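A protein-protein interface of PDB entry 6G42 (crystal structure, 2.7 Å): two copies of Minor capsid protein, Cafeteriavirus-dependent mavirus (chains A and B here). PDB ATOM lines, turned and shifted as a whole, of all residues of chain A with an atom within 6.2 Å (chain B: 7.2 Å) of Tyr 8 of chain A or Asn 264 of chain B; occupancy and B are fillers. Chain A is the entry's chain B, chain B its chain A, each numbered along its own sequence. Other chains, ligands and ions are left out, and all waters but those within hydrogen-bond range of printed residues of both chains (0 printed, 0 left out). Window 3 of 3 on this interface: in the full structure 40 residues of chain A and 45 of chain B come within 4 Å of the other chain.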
ATOM      1  N   LYS A   6     -14.867  16.152 -20.602  1.00  0.00           N
ATOM      2  CA  LYS A   6     -14.283  14.771 -20.631  1.00  0.00           C
ATOM      3  C   LYS A   6     -14.675  13.950 -19.398  1.00  0.00           C
ATOM      4  O   LYS A   6     -14.570  14.424 -18.263  1.00  0.00           O
ATOM      5  CB  LYS A   6     -12.755  14.814 -20.749  1.00  0.00           C
ATOM      6  CG  LYS A   6     -12.128  13.456 -21.036  1.00  0.00           C
ATOM      7  CD  LYS A   6     -10.681  13.589 -21.474  1.00  0.00           C
ATOM      8  CE  LYS A   6     -10.117  12.258 -21.946  1.00  0.00           C
ATOM      9  NZ  LYS A   6     -10.603  11.881 -23.299  1.00  0.00           N
ATOM     10  N   GLN A   7     -15.088  12.709 -19.636  1.00  0.00           N
ATOM     11  CA  GLN A   7     -15.643  11.838 -18.605  1.00  0.00           C
ATOM     12  C   GLN A   7     -14.899  10.500 -18.589  1.00  0.00           C
ATOM     13  O   GLN A   7     -14.676   9.900 -19.642  1.00  0.00           O
ATOM     14  CB  GLN A   7     -17.135  11.605 -18.874  1.00  0.00           C
ATOM     15  CG  GLN A   7     -17.920  11.018 -17.701  1.00  0.00           C
ATOM     16  CD  GLN A   7     -19.368  10.678 -18.050  1.00  0.00           C
ATOM     17  OE1 GLN A   7     -19.799  10.817 -19.200  1.00  0.00           O
ATOM     18  NE2 GLN A   7     -20.125  10.225 -17.052  1.00  0.00           N
ATOM     19  N   TYR A   8     -14.520  10.053 -17.390  1.00  0.00           N
ATOM     20  CA  TYR A   8     -13.885   8.753 -17.174  1.00  0.00           C
ATOM     21  C   TYR A   8     -14.841   7.889 -16.364  1.00  0.00           C
ATOM     22  O   TYR A   8     -15.117   8.190 -15.203  1.00  0.00           O
ATOM     23  CB  TYR A   8     -12.577   8.909 -16.396  1.00  0.00           C
ATOM     24  CG  TYR A   8     -11.478   9.615 -17.147  1.00  0.00           C
ATOM     25  CD1 TYR A   8     -11.458  11.002 -17.246  1.00  0.00           C
ATOM     26  CD2 TYR A   8     -10.450   8.901 -17.744  1.00  0.00           C
ATOM     27  CE1 TYR A   8     -10.447  11.657 -17.930  1.00  0.00           C
ATOM     28  CE2 TYR A   8      -9.436   9.545 -18.428  1.00  0.00           C
ATOM     29  CZ  TYR A   8      -9.439  10.922 -18.519  1.00  0.00           C
ATOM     30  OH  TYR A   8      -8.430  11.560 -19.198  1.00  0.00           O
ATOM     31  N   ILE A   9     -15.346   6.828 -16.982  1.00  0.00           N
ATOM     32  CA  ILE A   9     -16.241   5.887 -16.315  1.00  0.00           C
ATOM     33  C   ILE A   9     -15.470   4.583 -16.141  1.00  0.00           C
ATOM     34  O   ILE A   9     -15.029   3.981 -17.122  1.00  0.00           O
ATOM     35  CB  ILE A   9     -17.552   5.667 -17.115  1.00  0.00           C
ATOM     36  CG1 ILE A   9     -18.344   6.976 -17.209  1.00  0.00           C
ATOM     37  CG2 ILE A   9     -18.422   4.585 -16.476  1.00  0.00           C
ATOM     38  CD1 ILE A   9     -19.457   6.956 -18.247  1.00  0.00           C
ATOM     39  N   TRP A  10     -15.324   4.156 -14.889  1.00  0.00           N
ATOM     40  CA  TRP A  10     -14.586   2.945 -14.538  1.00  0.00           C
ATOM     41  C   TRP A  10     -15.542   1.825 -14.147  1.00  0.00           C
ATOM     42  O   TRP A  10     -16.557   2.073 -13.498  1.00  0.00           O
ATOM     43  CB  TRP A  10     -13.652   3.226 -13.366  1.00  0.00           C
ATOM     44  CG  TRP A  10     -12.626   4.271 -13.635  1.00  0.00           C
ATOM     45  CD1 TRP A  10     -12.703   5.593 -13.314  1.00  0.00           C
ATOM     46  CD2 TRP A  10     -11.354   4.082 -14.261  1.00  0.00           C
ATOM     47  NE1 TRP A  10     -11.564   6.245 -13.711  1.00  0.00           N
ATOM     48  CE2 TRP A  10     -10.714   5.339 -14.290  1.00  0.00           C
ATOM     49  CE3 TRP A  10     -10.692   2.970 -14.806  1.00  0.00           C
ATOM     50  CZ2 TRP A  10      -9.441   5.518 -14.842  1.00  0.00           C
ATOM     51  CZ3 TRP A  10      -9.426   3.146 -15.357  1.00  0.00           C
ATOM     52  CH2 TRP A  10      -8.814   4.413 -15.372  1.00  0.00           C
ATOM     53  N   LEU A 302     -12.054   1.007 -18.776  1.00  0.00           N
ATOM     54  CA  LEU A 302     -12.293   2.450 -18.803  1.00  0.00           C
ATOM     55  C   LEU A 302     -13.111   2.834 -20.042  1.00  0.00           C
ATOM     56  O   LEU A 302     -12.730   2.507 -21.165  1.00  0.00           O
ATOM     57  CB  LEU A 302     -10.965   3.218 -18.781  1.00  0.00           C
ATOM     58  CG  LEU A 302     -11.022   4.738 -19.024  1.00  0.00           C
ATOM     59  CD1 LEU A 302     -11.912   5.449 -18.011  1.00  0.00           C
ATOM     60  CD2 LEU A 302      -9.624   5.342 -19.025  1.00  0.00           C
ATOM     61  N   PHE A 303     -14.236   3.509 -19.819  1.00  0.00           N
ATOM     62  CA  PHE A 303     -14.976   4.191 -20.877  1.00  0.00           C
ATOM     63  C   PHE A 303     -14.612   5.674 -20.789  1.00  0.00           C
ATOM     64  O   PHE A 303     -14.956   6.345 -19.814  1.00  0.00           O
ATOM     65  CB  PHE A 303     -16.482   3.975 -20.722  1.00  0.00           C
ATOM     66  CG  PHE A 303     -16.902   2.526 -20.838  1.00  0.00           C
ATOM     67  CD1 PHE A 303     -17.203   1.970 -22.075  1.00  0.00           C
ATOM     68  CD2 PHE A 303     -16.990   1.716 -19.708  1.00  0.00           C
ATOM     69  CE1 PHE A 303     -17.580   0.637 -22.184  1.00  0.00           C
ATOM     70  CE2 PHE A 303     -17.370   0.381 -19.811  1.00  0.00           C
ATOM     71  CZ  PHE A 303     -17.664  -0.160 -21.050  1.00  0.00           C
ATOM     72  N   GLU A 304     -13.892   6.154 -21.802  1.00  0.00           N
ATOM     73  CA  GLU A 304     -13.335   7.510 -21.857  1.00  0.00           C
ATOM     74  C   GLU A 304     -14.038   8.264 -22.987  1.00  0.00           C
ATOM     75  O   GLU A 304     -14.009   7.821 -24.136  1.00  0.00           O
ATOM     76  CB  GLU A 304     -11.818   7.414 -22.114  1.00  0.00           C
ATOM     77  CG  GLU A 304     -11.022   8.720 -22.151  1.00  0.00           C
ATOM     78  CD  GLU A 304      -9.528   8.506 -22.451  1.00  0.00           C
ATOM     79  OE1 GLU A 304      -9.003   7.384 -22.257  1.00  0.00           O
ATOM     80  OE2 GLU A 304      -8.855   9.468 -22.887  1.00  0.00           O
ATOM     81  N   SER A 305     -14.675   9.388 -22.668  1.00  0.00           N
ATOM     82  CA  SER A 305     -15.411  10.163 -23.679  1.00  0.00           C
ATOM     83  C   SER A 305     -14.473  10.983 -24.574  1.00  0.00           C
ATOM     84  O   SER A 305     -13.332  11.246 -24.206  1.00  0.00           O
ATOM     85  CB  SER A 305     -16.449  11.070 -23.018  1.00  0.00           C
ATOM     86  OG  SER A 305     -15.826  12.136 -22.339  1.00  0.00           O
ATOM     87  N   ASN B  48     -13.828  23.033 -14.411  1.00  0.00           N
ATOM     88  CA  ASN B  48     -14.069  21.608 -14.154  1.00  0.00           C
ATOM     89  C   ASN B  48     -12.735  20.872 -14.032  1.00  0.00           C
ATOM     90  O   ASN B  48     -11.760  21.249 -14.679  1.00  0.00           O
ATOM     91  CB  ASN B  48     -14.913  21.007 -15.274  1.00  0.00           C
ATOM     92  CG  ASN B  48     -16.339  21.522 -15.265  1.00  0.00           C
ATOM     93  OD1 ASN B  48     -16.922  21.766 -14.205  1.00  0.00           O
ATOM     94  ND2 ASN B  48     -16.917  21.686 -16.451  1.00  0.00           N
ATOM     95  N   TYR B  49     -12.702  19.823 -13.209  1.00  0.00           N
ATOM     96  CA  TYR B  49     -11.445  19.181 -12.813  1.00  0.00           C
ATOM     97  C   TYR B  49     -11.444  17.656 -12.891  1.00  0.00           C
ATOM     98  O   TYR B  49     -12.476  17.005 -12.723  1.00  0.00           O
ATOM     99  CB  TYR B  49     -11.080  19.598 -11.383  1.00  0.00           C
ATOM    100  CG  TYR B  49     -10.763  21.069 -11.240  1.00  0.00           C
ATOM    101  CD1 TYR B  49     -11.773  21.994 -10.982  1.00  0.00           C
ATOM    102  CD2 TYR B  49      -9.452  21.540 -11.368  1.00  0.00           C
ATOM    103  CE1 TYR B  49     -11.488  23.345 -10.853  1.00  0.00           C
ATOM    104  CE2 TYR B  49      -9.161  22.892 -11.240  1.00  0.00           C
ATOM    105  CZ  TYR B  49     -10.188  23.789 -10.980  1.00  0.00           C
ATOM    106  OH  TYR B  49      -9.918  25.131 -10.845  1.00  0.00           O
ATOM    107  N   LEU B  50     -10.255  17.116 -13.155  1.00  0.00           N
ATOM    108  CA  LEU B  50      -9.943  15.706 -12.974  1.00  0.00           C
ATOM    109  C   LEU B  50      -9.061  15.577 -11.730  1.00  0.00           C
ATOM    110  O   LEU B  50      -8.327  16.508 -11.400  1.00  0.00           O
ATOM    111  CB  LEU B  50      -9.190  15.174 -14.192  1.00  0.00           C
ATOM    112  CG  LEU B  50      -9.893  15.282 -15.549  1.00  0.00           C
ATOM    113  CD1 LEU B  50      -8.956  14.870 -16.670  1.00  0.00           C
ATOM    114  CD2 LEU B  50     -11.161  14.437 -15.582  1.00  0.00           C
ATOM    115  N   LEU B  51      -9.144  14.430 -11.053  1.00  0.00           N
ATOM    116  CA  LEU B  51      -8.227  14.081  -9.957  1.00  0.00           C
ATOM    117  C   LEU B  51      -7.370  12.868 -10.305  1.00  0.00           C
ATOM    118  O   LEU B  51      -7.910  11.810 -10.648  1.00  0.00           O
ATOM    119  CB  LEU B  51      -8.992  13.768  -8.666  1.00  0.00           C
ATOM    120  CG  LEU B  51      -8.181  13.136  -7.518  1.00  0.00           C
ATOM    121  CD1 LEU B  51      -7.088  14.069  -7.031  1.00  0.00           C
ATOM    122  CD2 LEU B  51      -9.083  12.762  -6.366  1.00  0.00           C
ATOM    123  N   PRO B 212     -16.091  14.884  -3.265  1.00  0.00           N
ATOM    124  CA  PRO B 212     -17.072  14.791  -4.344  1.00  0.00           C
ATOM    125  C   PRO B 212     -16.403  14.392  -5.662  1.00  0.00           C
ATOM    126  O   PRO B 212     -15.943  15.243  -6.422  1.00  0.00           O
ATOM    127  CB  PRO B 212     -17.680  16.195  -4.387  1.00  0.00           C
ATOM    128  CG  PRO B 212     -16.594  17.089  -3.906  1.00  0.00           C
ATOM    129  CD  PRO B 212     -15.800  16.289  -2.913  1.00  0.00           C
ATOM    130  N   VAL B 213     -16.359  13.084  -5.896  1.00  0.00           N
ATOM    131  CA  VAL B 213     -15.667  12.478  -7.029  1.00  0.00           C
ATOM    132  C   VAL B 213     -16.538  11.345  -7.587  1.00  0.00           C
ATOM    133  O   VAL B 213     -17.289  10.713  -6.842  1.00  0.00           O
ATOM    134  CB  VAL B 213     -14.266  11.957  -6.598  1.00  0.00           C
ATOM    135  CG1 VAL B 213     -14.370  10.812  -5.598  1.00  0.00           C
ATOM    136  CG2 VAL B 213     -13.427  11.536  -7.797  1.00  0.00           C
ATOM    137  N   SER B 214     -16.430  11.091  -8.890  1.00  0.00           N
ATOM    138  CA  SER B 214     -17.184  10.008  -9.539  1.00  0.00           C
ATOM    139  C   SER B 214     -16.772   8.654  -8.978  1.00  0.00           C
ATOM    140  O   SER B 214     -15.584   8.356  -8.882  1.00  0.00           O
ATOM    141  CB  SER B 214     -16.977  10.011 -11.060  1.00  0.00           C
ATOM    142  OG  SER B 214     -17.869  10.903 -11.709  1.00  0.00           O
ATOM    143  N   TYR B 215     -17.761   7.845  -8.615  1.00  0.00           N
ATOM    144  CA  TYR B 215     -17.527   6.517  -8.049  1.00  0.00           C
ATOM    145  C   TYR B 215     -17.150   5.549  -9.181  1.00  0.00           C
ATOM    146  O   TYR B 215     -17.487   5.773 -10.340  1.00  0.00           O
ATOM    147  CB  TYR B 215     -18.792   5.999  -7.345  1.00  0.00           C
ATOM    148  CG  TYR B 215     -19.129   6.600  -5.978  1.00  0.00           C
ATOM    149  CD1 TYR B 215     -19.117   7.985  -5.757  1.00  0.00           C
ATOM    150  CD2 TYR B 215     -19.513   5.776  -4.906  1.00  0.00           C
ATOM    151  CE1 TYR B 215     -19.444   8.523  -4.514  1.00  0.00           C
ATOM    152  CE2 TYR B 215     -19.840   6.306  -3.662  1.00  0.00           C
ATOM    153  CZ  TYR B 215     -19.804   7.677  -3.469  1.00  0.00           C
ATOM    154  OH  TYR B 215     -20.124   8.205  -2.239  1.00  0.00           O
ATOM    155  N   SER B 259      -0.606   8.691 -17.853  1.00  0.00           N
ATOM    156  CA  SER B 259      -1.551   7.745 -17.248  1.00  0.00           C
ATOM    157  C   SER B 259      -2.990   8.093 -17.625  1.00  0.00           C
ATOM    158  O   SER B 259      -3.303   9.252 -17.914  1.00  0.00           O
ATOM    159  CB  SER B 259      -1.417   7.727 -15.726  1.00  0.00           C
ATOM    160  OG  SER B 259      -2.183   6.670 -15.173  1.00  0.00           O
ATOM    161  N   ASN B 260      -3.851   7.074 -17.613  1.00  0.00           N
ATOM    162  CA  ASN B 260      -5.302   7.242 -17.769  1.00  0.00           C
ATOM    163  C   ASN B 260      -6.043   7.318 -16.425  1.00  0.00           C
ATOM    164  O   ASN B 260      -7.261   7.509 -16.423  1.00  0.00           O
ATOM    165  CB  ASN B 260      -5.900   6.070 -18.561  1.00  0.00           C
ATOM    166  CG  ASN B 260      -5.325   5.937 -19.958  1.00  0.00           C
ATOM    167  OD1 ASN B 260      -5.138   6.927 -20.661  1.00  0.00           O
ATOM    168  ND2 ASN B 260      -5.068   4.703 -20.380  1.00  0.00           N
ATOM    169  N   LYS B 261      -5.331   7.194 -15.296  1.00  0.00           N
ATOM    170  CA  LYS B 261      -5.960   6.965 -13.975  1.00  0.00           C
ATOM    171  C   LYS B 261      -6.555   8.228 -13.340  1.00  0.00           C
ATOM    172  O   LYS B 261      -6.185   8.622 -12.229  1.00  0.00           O
ATOM    173  CB  LYS B 261      -4.956   6.322 -13.017  1.00  0.00           C
ATOM    174  CG  LYS B 261      -4.426   4.976 -13.481  1.00  0.00           C
ATOM    175  CD  LYS B 261      -3.407   4.404 -12.501  1.00  0.00           C
ATOM    176  CE  LYS B 261      -4.072   3.729 -11.304  1.00  0.00           C
ATOM    177  NZ  LYS B 261      -4.656   2.400 -11.646  1.00  0.00           N
ATOM    178  N   TYR B 262      -7.503   8.833 -14.051  1.00  0.00           N
ATOM    179  CA  TYR B 262      -8.160  10.069 -13.632  1.00  0.00           C
ATOM    180  C   TYR B 262      -9.584   9.764 -13.163  1.00  0.00           C
ATOM    181  O   TYR B 262     -10.202   8.788 -13.595  1.00  0.00           O
ATOM    182  CB  TYR B 262      -8.228  11.072 -14.789  1.00  0.00           C
ATOM    183  CG  TYR B 262      -6.923  11.733 -15.192  1.00  0.00           C
ATOM    184  CD1 TYR B 262      -6.399  12.800 -14.462  1.00  0.00           C
ATOM    185  CD2 TYR B 262      -6.244  11.330 -16.342  1.00  0.00           C
ATOM    186  CE1 TYR B 262      -5.215  13.423 -14.843  1.00  0.00           C
ATOM    187  CE2 TYR B 262      -5.064  11.947 -16.736  1.00  0.00           C
ATOM    188  CZ  TYR B 262      -4.553  12.990 -15.986  1.00  0.00           C
ATOM    189  OH  TYR B 262      -3.382  13.593 -16.384  1.00  0.00           O
ATOM    190  N   HIS B 263     -10.090  10.620 -12.278  1.00  0.00           N
ATOM    191  CA  HIS B 263     -11.475  10.573 -11.816  1.00  0.00           C
ATOM    192  C   HIS B 263     -12.074  11.962 -11.925  1.00  0.00           C
ATOM    193  O   HIS B 263     -11.372  12.959 -11.746  1.00  0.00           O
ATOM    194  CB  HIS B 263     -11.528  10.085 -10.377  1.00  0.00           C
ATOM    195  CG  HIS B 263     -10.852   8.768 -10.176  1.00  0.00           C
ATOM    196  ND1 HIS B 263     -11.464   7.569 -10.465  1.00  0.00           N
ATOM    197  CD2 HIS B 263      -9.603   8.463  -9.750  1.00  0.00           C
ATOM    198  CE1 HIS B 263     -10.627   6.581 -10.210  1.00  0.00           C
ATOM    199  NE2 HIS B 263      -9.491   7.094  -9.774  1.00  0.00           N
ATOM    200  N   ASN B 264     -13.366  12.029 -12.233  1.00  0.00           N
ATOM    201  CA  ASN B 264     -14.058  13.314 -12.364  1.00  0.00           C
ATOM    202  C   ASN B 264     -14.439  13.860 -10.998  1.00  0.00           C
ATOM    203  O   ASN B 264     -15.052  13.152 -10.195  1.00  0.00           O
ATOM    204  CB  ASN B 264     -15.322  13.180 -13.220  1.00  0.00           C
ATOM    205  CG  ASN B 264     -15.013  12.969 -14.686  1.00  0.00           C
ATOM    206  OD1 ASN B 264     -15.302  11.906 -15.243  1.00  0.00           O
ATOM    207  ND2 ASN B 264     -14.414  13.977 -15.321  1.00  0.00           N
ATOM    208  N   ILE B 265     -14.067  15.116 -10.750  1.00  0.00           N
ATOM    209  CA  ILE B 265     -14.564  15.874  -9.607  1.00  0.00           C
ATOM    210  C   ILE B 265     -15.937  16.434  -9.993  1.00  0.00           C
ATOM    211  O   ILE B 265     -16.056  17.159 -10.978  1.00  0.00           O
ATOM    212  CB  ILE B 265     -13.595  17.013  -9.220  1.00  0.00           C
ATOM    213  CG1 ILE B 265     -12.212  16.453  -8.839  1.00  0.00           C
ATOM    214  CG2 ILE B 265     -14.154  17.859  -8.076  1.00  0.00           C
ATOM    215  CD1 ILE B 265     -12.197  15.500  -7.651  1.00  0.00           C
ATOM    216  N   LEU B 266     -16.955  16.092  -9.205  1.00  0.00           N
ATOM    217  CA  LEU B 266     -18.349  16.474  -9.476  1.00  0.00           C
ATOM    218  C   LEU B 266     -18.766  17.839  -8.902  1.00  0.00           C
ATOM    219  O   LEU B 266     -19.604  18.522  -9.492  1.00  0.00           O
ATOM    220  CB  LEU B 266     -19.292  15.394  -8.942  1.00  0.00           C
ATOM    221  CG  LEU B 266     -19.106  13.986  -9.514  1.00  0.00           C
ATOM    222  CD1 LEU B 266     -19.999  12.992  -8.782  1.00  0.00           C
ATOM    223  CD2 LEU B 266     -19.383  13.955 -11.013  1.00  0.00           C
ATOM    224  N   GLN B 267     -18.197  18.217  -7.757  1.00  0.00           N
ATOM    225  CA  GLN B 267     -18.482  19.498  -7.099  1.00  0.00           C
ATOM    226  C   GLN B 267     -17.180  20.226  -6.793  1.00  0.00           C
ATOM    227  O   GLN B 267     -16.294  19.653  -6.182  1.00  0.00           O
ATOM    228  CB  GLN B 267     -19.227  19.265  -5.786  1.00  0.00           C
ATOM    229  CG  GLN B 267     -20.602  18.631  -5.927  1.00  0.00           C
ATOM    230  CD  GLN B 267     -21.675  19.648  -6.262  1.00  0.00           C
ATOM    231  OE1 GLN B 267     -21.708  20.182  -7.370  1.00  0.00           O
ATOM    232  NE2 GLN B 267     -22.559  19.927  -5.302  1.00  0.00           N
ATOM    233  N   GLU B 304      -6.396  18.628 -12.012  1.00  0.00           N
ATOM    234  CA  GLU B 304      -6.039  19.132 -13.340  1.00  0.00           C
ATOM    235  C   GLU B 304      -7.318  19.568 -14.047  1.00  0.00           C
ATOM    236  O   GLU B 304      -8.235  18.762 -14.198  1.00  0.00           O
ATOM    237  CB  GLU B 304      -5.345  18.016 -14.124  1.00  0.00           C
ATOM    238  CG  GLU B 304      -4.810  18.375 -15.507  1.00  0.00           C
ATOM    239  CD  GLU B 304      -4.273  17.156 -16.254  1.00  0.00           C
ATOM    240  OE1 GLU B 304      -3.752  16.217 -15.605  1.00  0.00           O
ATOM    241  OE2 GLU B 304      -4.375  17.130 -17.498  1.00  0.00           O
ATOM    242  N   ILE B 306      -9.820  20.945 -17.179  1.00  0.00           N
ATOM    243  CA  ILE B 306     -10.083  20.483 -18.549  1.00  0.00           C
ATOM    244  C   ILE B 306     -10.397  21.676 -19.458  1.00  0.00           C
ATOM    245  O   ILE B 306     -11.498  22.231 -19.424  1.00  0.00           O
ATOM    246  CB  ILE B 306     -11.249  19.462 -18.597  1.00  0.00           C
ATOM    247  CG1 ILE B 306     -11.099  18.403 -17.497  1.00  0.00           C
ATOM    248  CG2 ILE B 306     -11.306  18.789 -19.968  1.00  0.00           C
ATOM    249  CD1 ILE B 306     -12.324  17.532 -17.310  1.00  0.00           C
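O of Lys 6 of chain A is in hydrogen-bond range of ND2 of Asn 264 of chain B, 3.0 Å away. NE1 of Trp 10 of chain A lies within hydrogen-bond range of O of Tyr 262 of chain B (2.9 Å). OD1 of Asn 264 of chain B lies within hydrogen-bond range of N of Tyr 8 of chain A (2.9 Å).
The backbone carbonyl oxygen (O) of Glu 304 of chain B lies within hydrogen-bond range of the backbone NH (N) of Leu 50 of chain B (2.8 Å). OG of Ser 259 of chain B is in hydrogen-bond range of N of Lys 261 of chain B (3.2 Å). The backbone NH (N) of Ile 306 of chain B lies within hydrogen-bond range of the backbone carbonyl oxygen (O) of Asn 48 of chain B, 3.2 Å away. N of Leu 51 of chain B is in hydrogen-bond range of O of His 263 of chain B (2.8 Å). The side-chain carboxylate (OE1) of Glu 304 of chain B sits at hydrogen-bond distance from the side-chain hydroxyl (OH) of Tyr 262 of chain B. N of Gln 7 of chain A sits at hydrogen-bond distance from OG of Ser 305 of chain A.
Among the printed residues, pairs that only touch across the chains: Trp 10 of chain A with Asn 260 of chain B (3.3 Å), Gln 7 of chain A with Asn 264 of chain B (3.4 Å), Trp 10 of chain A with His 263 of chain B (3.5 Å), Tyr 8 of chain A with Asn 260 of chain B (3.6 Å), Tyr 8 of chain A with Tyr 262 of chain B (3.6 Å), Tyr 8 of chain A with Leu 50 of chain B (3.7 Å), Leu 302 of chain A with Asn 260 of chain B (3.8 Å), Trp 10 of chain A with Lys 261 of chain B (3.9 Å) and Lys 6 of chain A with Ile 306 of chain B (3.95 Å).
Tyr 8 of chain A touches four residues of chain B. Glu 304 of chain A touches none of the printed residues of chain B. Of the printed residues of chain A, Leu 50 of chain B touches Tyr 8 (3.7 Å). Printed residues of chain A within 4 Å of Asn 260 of chain B: Tyr 8 (3.6 Å), Trp 10 (3.3 Å) and Leu 302 (3.8 Å). Printed residues of chain A within 4 Å of Tyr 262 of chain B: Tyr 8 (3.6 Å) and Trp 10 (2.9 Å). Of the printed residues of chain A, His 263 of chain B touches Trp 10. Asn 264 of chain B touches just these residues of chain A: Lys 6 (3.0 Å), Gln 7 (3.4 Å) and Tyr 8 (2.9 Å). Printed residues of chain A within 4 Å of Ile 306 of chain B: Lys 6. The nearest residue of chain A that does not touch Asn 264 of chain B is Ile 9 of chain A (5.4 Å). The nearest printed residue of chain A that does not touch Ile 306 of chain B is Gln 7 of chain A (6.0 Å).
Hydrophobic or aromatic side chains of chain A within 4 Å of the printed part of chain B: Tyr 8, Trp 10 and Leu 302. Among the printed residues, 12 pairs touch across the chains.
Position printed for both chains: 304.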
